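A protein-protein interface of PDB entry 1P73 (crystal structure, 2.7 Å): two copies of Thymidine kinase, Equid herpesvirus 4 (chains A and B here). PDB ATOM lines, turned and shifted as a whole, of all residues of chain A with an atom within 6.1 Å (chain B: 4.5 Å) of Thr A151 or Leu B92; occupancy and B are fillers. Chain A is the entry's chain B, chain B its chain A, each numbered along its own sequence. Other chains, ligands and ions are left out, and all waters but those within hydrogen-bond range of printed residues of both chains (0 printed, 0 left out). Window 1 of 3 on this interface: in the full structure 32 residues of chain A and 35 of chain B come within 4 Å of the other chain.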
ATOM      1  N   THR A  88      -6.766  16.003  -8.500  1.00  0.00           N
ATOM      2  CA  THR A  88      -7.510  14.797  -8.234  1.00  0.00           C
ATOM      3  C   THR A  88      -6.722  13.507  -8.417  1.00  0.00           C
ATOM      4  O   THR A  88      -6.864  12.576  -7.616  1.00  0.00           O
ATOM      5  CB  THR A  88      -8.730  14.790  -9.118  1.00  0.00           C
ATOM      6  OG1 THR A  88      -9.728  15.617  -8.516  1.00  0.00           O
ATOM      7  CG2 THR A  88      -9.378  13.443  -9.100  1.00  0.00           C
ATOM      8  N   LEU A  92      -7.311   9.664  -6.397  1.00  0.00           N
ATOM      9  CA  LEU A  92      -7.989   8.571  -7.081  1.00  0.00           C
ATOM     10  C   LEU A  92      -7.153   7.294  -7.079  1.00  0.00           C
ATOM     11  O   LEU A  92      -7.664   6.186  -6.894  1.00  0.00           O
ATOM     12  CB  LEU A  92      -8.277   8.984  -8.527  1.00  0.00           C
ATOM     13  CG  LEU A  92      -9.352  10.053  -8.737  1.00  0.00           C
ATOM     14  CD1 LEU A  92      -9.686  10.188 -10.219  1.00  0.00           C
ATOM     15  CD2 LEU A  92     -10.621   9.751  -7.883  1.00  0.00           C
ATOM     16  N   THR A 127     -12.675  16.608  -6.215  1.00  0.00           N
ATOM     17  CA  THR A 127     -13.668  16.357  -7.251  1.00  0.00           C
ATOM     18  C   THR A 127     -14.959  17.123  -7.021  1.00  0.00           C
ATOM     19  O   THR A 127     -15.685  17.401  -7.978  1.00  0.00           O
ATOM     20  CB  THR A 127     -13.952  14.837  -7.421  1.00  0.00           C
ATOM     21  OG1 THR A 127     -14.534  14.313  -6.219  1.00  0.00           O
ATOM     22  CG2 THR A 127     -12.638  14.042  -7.609  1.00  0.00           C
ATOM     23  N   MET A 146     -19.423  19.528 -13.539  1.00  0.00           N
ATOM     24  CA  MET A 146     -19.968  18.212 -13.779  1.00  0.00           C
ATOM     25  C   MET A 146     -18.870  17.255 -14.228  1.00  0.00           C
ATOM     26  O   MET A 146     -18.884  16.093 -13.834  1.00  0.00           O
ATOM     27  CB  MET A 146     -21.099  18.286 -14.798  1.00  0.00           C
ATOM     28  CG  MET A 146     -22.395  18.879 -14.226  1.00  0.00           C
ATOM     29  SD  MET A 146     -23.242  17.718 -13.148  1.00  0.00           S
ATOM     30  CE  MET A 146     -24.888  17.750 -13.836  1.00  0.00           C
ATOM     31  N   ALA A 147     -17.911  17.746 -15.020  1.00  0.00           N
ATOM     32  CA  ALA A 147     -16.767  16.929 -15.420  1.00  0.00           C
ATOM     33  C   ALA A 147     -16.000  16.439 -14.209  1.00  0.00           C
ATOM     34  O   ALA A 147     -15.688  15.261 -14.131  1.00  0.00           O
ATOM     35  CB  ALA A 147     -15.847  17.663 -16.368  1.00  0.00           C
ATOM     36  N   MET A 148     -15.718  17.343 -13.267  1.00  0.00           N
ATOM     37  CA  MET A 148     -15.070  17.021 -11.992  1.00  0.00           C
ATOM     38  C   MET A 148     -15.923  16.087 -11.120  1.00  0.00           C
ATOM     39  O   MET A 148     -15.472  15.015 -10.725  1.00  0.00           O
ATOM     40  CB  MET A 148     -14.779  18.303 -11.204  1.00  0.00           C
ATOM     41  CG  MET A 148     -13.820  19.285 -11.841  1.00  0.00           C
ATOM     42  SD  MET A 148     -12.213  18.573 -12.284  1.00  0.00           S
ATOM     43  CE  MET A 148     -11.771  17.493 -10.773  1.00  0.00           C
ATOM     44  N   VAL A 149     -17.158  16.502 -10.836  1.00  0.00           N
ATOM     45  CA  VAL A 149     -18.056  15.766  -9.939  1.00  0.00           C
ATOM     46  C   VAL A 149     -18.292  14.312 -10.383  1.00  0.00           C
ATOM     47  O   VAL A 149     -18.409  13.429  -9.535  1.00  0.00           O
ATOM     48  CB  VAL A 149     -19.435  16.519  -9.708  1.00  0.00           C
ATOM     49  CG1 VAL A 149     -20.480  15.597  -9.066  1.00  0.00           C
ATOM     50  CG2 VAL A 149     -19.255  17.799  -8.864  1.00  0.00           C
ATOM     51  N   ALA A 150     -18.354  14.062 -11.692  1.00  0.00           N
ATOM     52  CA  ALA A 150     -18.596  12.708 -12.191  1.00  0.00           C
ATOM     53  C   ALA A 150     -17.453  11.752 -11.864  1.00  0.00           C
ATOM     54  O   ALA A 150     -17.658  10.534 -11.836  1.00  0.00           O
ATOM     55  CB  ALA A 150     -18.853  12.714 -13.652  1.00  0.00           C
ATOM     56  N   THR A 151     -16.266  12.292 -11.595  1.00  0.00           N
ATOM     57  CA  THR A 151     -15.091  11.470 -11.334  1.00  0.00           C
ATOM     58  C   THR A 151     -14.911  11.134  -9.854  1.00  0.00           C
ATOM     59  O   THR A 151     -13.905  10.537  -9.471  1.00  0.00           O
ATOM     60  CB  THR A 151     -13.815  12.151 -11.849  1.00  0.00           C
ATOM     61  OG1 THR A 151     -13.606  13.340 -11.100  1.00  0.00           O
ATOM     62  CG2 THR A 151     -13.984  12.667 -13.270  1.00  0.00           C
ATOM     63  N   LEU A 152     -15.858  11.528  -9.011  1.00  0.00           N
ATOM     64  CA  LEU A 152     -15.793  11.134  -7.611  1.00  0.00           C
ATOM     65  C   LEU A 152     -16.037   9.614  -7.556  1.00  0.00           C
ATOM     66  O   LEU A 152     -16.955   9.115  -8.201  1.00  0.00           O
ATOM     67  CB  LEU A 152     -16.822  11.920  -6.790  1.00  0.00           C
ATOM     68  CG  LEU A 152     -17.298  11.401  -5.432  1.00  0.00           C
ATOM     69  CD1 LEU A 152     -16.305  11.717  -4.313  1.00  0.00           C
ATOM     70  CD2 LEU A 152     -18.654  11.969  -5.079  1.00  0.00           C
ATOM     71  N   PRO A 153     -15.205   8.866  -6.836  1.00  0.00           N
ATOM     72  CA  PRO A 153     -15.398   7.413  -6.755  1.00  0.00           C
ATOM     73  C   PRO A 153     -16.367   7.048  -5.626  1.00  0.00           C
ATOM     74  O   PRO A 153     -16.535   7.835  -4.701  1.00  0.00           O
ATOM     75  CB  PRO A 153     -13.988   6.897  -6.464  1.00  0.00           C
ATOM     76  CG  PRO A 153     -13.311   8.030  -5.703  1.00  0.00           C
ATOM     77  CD  PRO A 153     -14.023   9.308  -6.068  1.00  0.00           C
ATOM     78  N   ALA A 275     -25.916   9.616  -8.698  1.00  0.00           N
ATOM     79  CA  ALA A 275     -24.559   9.085  -8.507  1.00  0.00           C
ATOM     80  C   ALA A 275     -23.820   9.748  -7.343  1.00  0.00           C
ATOM     81  O   ALA A 275     -23.093   9.082  -6.614  1.00  0.00           O
ATOM     82  CB  ALA A 275     -23.734   9.184  -9.801  1.00  0.00           C
ATOM     83  N   LYS A 279     -22.667   7.767  -3.881  1.00  0.00           N
ATOM     84  CA  LYS A 279     -21.239   7.848  -3.600  1.00  0.00           C
ATOM     85  C   LYS A 279     -20.887   8.401  -2.222  1.00  0.00           C
ATOM     86  O   LYS A 279     -19.826   8.078  -1.687  1.00  0.00           O
ATOM     87  CB  LYS A 279     -20.512   8.625  -4.698  1.00  0.00           C
ATOM     88  CG  LYS A 279     -20.420   7.850  -6.012  1.00  0.00           C
ATOM     89  CD  LYS A 279     -19.786   8.694  -7.094  1.00  0.00           C
ATOM     90  CE  LYS A 279     -20.192   8.244  -8.484  1.00  0.00           C
ATOM     91  NZ  LYS A 279     -19.647   9.188  -9.488  1.00  0.00           N
ATOM     92  N   THR B  88     -15.759  12.270 -21.523  1.00  0.00           N
ATOM     93  CA  THR B  88     -15.895  11.208 -20.537  1.00  0.00           C
ATOM     94  C   THR B  88     -17.124  11.396 -19.653  1.00  0.00           C
ATOM     95  O   THR B  88     -17.826  10.440 -19.353  1.00  0.00           O
ATOM     96  CB  THR B  88     -14.605  11.182 -19.688  1.00  0.00           C
ATOM     97  OG1 THR B  88     -13.544  10.585 -20.442  1.00  0.00           O
ATOM     98  CG2 THR B  88     -14.748  10.288 -18.485  1.00  0.00           C
ATOM     99  N   THR B  89     -17.382  12.629 -19.234  1.00  0.00           N
ATOM    100  CA  THR B  89     -18.502  12.923 -18.326  1.00  0.00           C
ATOM    101  C   THR B  89     -19.798  12.103 -18.550  1.00  0.00           C
ATOM    102  O   THR B  89     -20.193  11.358 -17.668  1.00  0.00           O
ATOM    103  CB  THR B  89     -18.786  14.439 -18.260  1.00  0.00           C
ATOM    104  OG1 THR B  89     -17.554  15.129 -18.017  1.00  0.00           O
ATOM    105  CG2 THR B  89     -19.645  14.775 -17.035  1.00  0.00           C
ATOM    106  N   PRO B  90     -20.458  12.212 -19.697  1.00  0.00           N
ATOM    107  CA  PRO B  90     -21.717  11.482 -19.877  1.00  0.00           C
ATOM    108  C   PRO B  90     -21.536   9.956 -19.807  1.00  0.00           C
ATOM    109  O   PRO B  90     -22.496   9.241 -19.483  1.00  0.00           O
ATOM    110  CB  PRO B  90     -22.191  11.928 -21.264  1.00  0.00           C
ATOM    111  CG  PRO B  90     -20.970  12.385 -21.976  1.00  0.00           C
ATOM    112  CD  PRO B  90     -20.107  12.995 -20.898  1.00  0.00           C
ATOM    113  N   TYR B  91     -20.327   9.467 -20.087  1.00  0.00           N
ATOM    114  CA  TYR B  91     -20.048   8.033 -19.971  1.00  0.00           C
ATOM    115  C   TYR B  91     -20.033   7.584 -18.512  1.00  0.00           C
ATOM    116  O   TYR B  91     -20.662   6.587 -18.173  1.00  0.00           O
ATOM    117  CB  TYR B  91     -18.761   7.636 -20.719  1.00  0.00           C
ATOM    118  CG  TYR B  91     -19.004   7.455 -22.202  1.00  0.00           C
ATOM    119  CD1 TYR B  91     -19.825   6.407 -22.667  1.00  0.00           C
ATOM    120  CD2 TYR B  91     -18.477   8.337 -23.136  1.00  0.00           C
ATOM    121  CE1 TYR B  91     -20.096   6.235 -24.020  1.00  0.00           C
ATOM    122  CE2 TYR B  91     -18.742   8.171 -24.504  1.00  0.00           C
ATOM    123  CZ  TYR B  91     -19.552   7.115 -24.933  1.00  0.00           C
ATOM    124  OH  TYR B  91     -19.832   6.912 -26.272  1.00  0.00           O
ATOM    125  N   LEU B  92     -19.355   8.339 -17.649  1.00  0.00           N
ATOM    126  CA  LEU B  92     -19.390   8.070 -16.215  1.00  0.00           C
ATOM    127  C   LEU B  92     -20.803   8.156 -15.642  1.00  0.00           C
ATOM    128  O   LEU B  92     -21.167   7.381 -14.752  1.00  0.00           O
ATOM    129  CB  LEU B  92     -18.425   8.978 -15.439  1.00  0.00           C
ATOM    130  CG  LEU B  92     -16.975   9.112 -15.923  1.00  0.00           C
ATOM    131  CD1 LEU B  92     -16.206  10.164 -15.126  1.00  0.00           C
ATOM    132  CD2 LEU B  92     -16.233   7.795 -15.909  1.00  0.00           C
ATOM    133  N   ILE B  93     -21.607   9.080 -16.153  1.00  0.00           N
ATOM    134  CA  ILE B  93     -22.994   9.195 -15.715  1.00  0.00           C
ATOM    135  C   ILE B  93     -23.837   7.992 -16.127  1.00  0.00           C
ATOM    136  O   ILE B  93     -24.551   7.418 -15.289  1.00  0.00           O
ATOM    137  CB  ILE B  93     -23.641  10.525 -16.176  1.00  0.00           C
ATOM    138  CG1 ILE B  93     -22.934  11.726 -15.537  1.00  0.00           C
ATOM    139  CG2 ILE B  93     -25.112  10.553 -15.815  1.00  0.00           C
ATOM    140  CD1 ILE B  93     -23.059  12.993 -16.353  1.00  0.00           C
ATOM    141  N   LEU B  94     -23.761   7.603 -17.398  1.00  0.00           N
ATOM    142  CA  LEU B  94     -24.471   6.393 -17.845  1.00  0.00           C
ATOM    143  C   LEU B  94     -23.991   5.108 -17.138  1.00  0.00           C
ATOM    144  O   LEU B  94     -24.810   4.295 -16.735  1.00  0.00           O
ATOM    145  CB  LEU B  94     -24.452   6.244 -19.381  1.00  0.00           C
ATOM    146  CG  LEU B  94     -25.300   5.101 -19.971  1.00  0.00           C
ATOM    147  CD1 LEU B  94     -26.783   5.254 -19.609  1.00  0.00           C
ATOM    148  CD2 LEU B  94     -25.135   4.983 -21.470  1.00  0.00           C
ATOM    149  N   HIS B  95     -22.676   4.938 -16.971  1.00  0.00           N
ATOM    150  CA  HIS B  95     -22.121   3.798 -16.223  1.00  0.00           C
ATOM    151  C   HIS B  95     -22.639   3.711 -14.790  1.00  0.00           C
ATOM    152  O   HIS B  95     -23.008   2.640 -14.335  1.00  0.00           O
ATOM    153  CB  HIS B  95     -20.585   3.834 -16.211  1.00  0.00           C
ATOM    154  CG  HIS B  95     -19.935   2.480 -16.098  1.00  0.00           C
ATOM    155  ND1 HIS B  95     -19.526   1.946 -14.892  1.00  0.00           N
ATOM    156  CD2 HIS B  95     -19.587   1.575 -17.046  1.00  0.00           C
ATOM    157  CE1 HIS B  95     -18.954   0.774 -15.103  1.00  0.00           C
ATOM    158  NE2 HIS B  95     -18.982   0.523 -16.401  1.00  0.00           N
ATOM    159  N   ASP B  96     -22.668   4.830 -14.078  1.00  0.00           N
ATOM    160  CA  ASP B  96     -23.165   4.837 -12.701  1.00  0.00           C
ATOM    161  C   ASP B  96     -24.647   4.473 -12.572  1.00  0.00           C
ATOM    162  O   ASP B  96     -25.058   3.872 -11.575  1.00  0.00           O
ATOM    163  CB  ASP B  96     -22.937   6.194 -12.056  1.00  0.00           C
ATOM    164  CG  ASP B  96     -21.512   6.408 -11.651  1.00  0.00           C
ATOM    165  OD1 ASP B  96     -20.854   5.417 -11.249  1.00  0.00           O
ATOM    166  OD2 ASP B  96     -20.968   7.539 -11.701  1.00  0.00           O
ATOM    167  N   THR B 151      -9.670   7.830 -14.036  1.00  0.00           N
ATOM    168  CA  THR B 151     -11.111   8.067 -13.956  1.00  0.00           C
ATOM    169  C   THR B 151     -11.924   6.971 -14.613  1.00  0.00           C
ATOM    170  O   THR B 151     -13.167   6.992 -14.544  1.00  0.00           O
ATOM    171  CB  THR B 151     -11.517   9.422 -14.578  1.00  0.00           C
ATOM    172  OG1 THR B 151     -11.293   9.380 -15.992  1.00  0.00           O
ATOM    173  CG2 THR B 151     -10.642  10.581 -14.064  1.00  0.00           C
ATOM    174  N   PRO B 153     -13.944   3.971 -14.747  1.00  0.00           N
ATOM    175  CA  PRO B 153     -14.737   3.207 -13.765  1.00  0.00           C
ATOM    176  C   PRO B 153     -14.473   1.694 -13.812  1.00  0.00           C
ATOM    177  O   PRO B 153     -14.111   1.149 -14.862  1.00  0.00           O
ATOM    178  CB  PRO B 153     -16.186   3.508 -14.162  1.00  0.00           C
ATOM    179  CG  PRO B 153     -16.131   3.909 -15.583  1.00  0.00           C
ATOM    180  CD  PRO B 153     -14.789   4.568 -15.797  1.00  0.00           C
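The side-chain carboxylate (OD2) of Asp B96 is in salt-bridge range of the side-chain amino group (NZ) of Lys A279 (3.1 Å).
NZ of Lys A279 sits at hydrogen-bond distance from O of Leu A152 (3.0 Å). The side-chain amino group (NZ) of Lys A279 sits at hydrogen-bond distance from the backbone carbonyl oxygen (O) of Ala A150 (3.4 Å). The backbone carbonyl oxygen of Met A148 sits at hydrogen-bond distance from the side-chain hydroxyl of Thr A151 (2.5 Å).
CG2 of Thr B151 touches CD1 of Leu A92, at 3.98 Å. O of Met A146 touches CG2 of Thr B89 (3.5 Å). Thr B89 touches Ala A147. Leu B92 touches Ala A150 (CD1 to O, 3.6 Å). Leu B92 touches Thr A151 (CD1 to CG2, 3.8 Å). Ala A275 touches Asp B96.
Printed residues of chain B within 4 Å of Thr A151: Leu B92 (3.8 Å). Of chain A, only Ala A150 and Thr A151 come within 4 Å of Leu B92. Of the printed residues of chain A, Thr B89 touches Met A146 and Ala A147. Of the printed residues of chain A, Asp B96 touches Ala A275 and Lys A279. Val A149 touches none of the printed residues of chain B. The nearest printed residue of chain B that does not touch Thr A151 is Thr B151 (4.02 Å). The nearest residue of chain A that does not touch Leu B92 is Ala A147 (5.2 Å). The nearest printed residue of chain B that does not touch Lys A279 is Leu B92 (5.8 Å).
Of the 13 printed residues of chain A, 7 touch a printed residue of chain B. Printed residues of chain A that touch a printed residue of chain B: Leu A92, Met A146, Ala A147, Ala A150, Thr A151, Ala A275 and Lys A279. Hydrophobic or aromatic side chains of chain A within 4 Å of the printed part of chain B: Leu A92, Ala A147, Ala A150 and Ala A275. Hydrophobic or aromatic side chains of chain B within 4 Å of the printed part of chain A: Leu B92. Among the printed residues, 7 pairs touch across the chains. Among the printed residues, Asp or Glu carboxylates within 4 Å of a Lys or Arg side-chain nitrogen of the other chain: Lys A279 with Asp B96.
Leu A92 touches Thr B151, and with the chains exchanged Thr A151 touches Leu B92. Of the 7 pairs that touch across the chains among the printed residues, 2 have their exchanged pair printed and touching as well.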
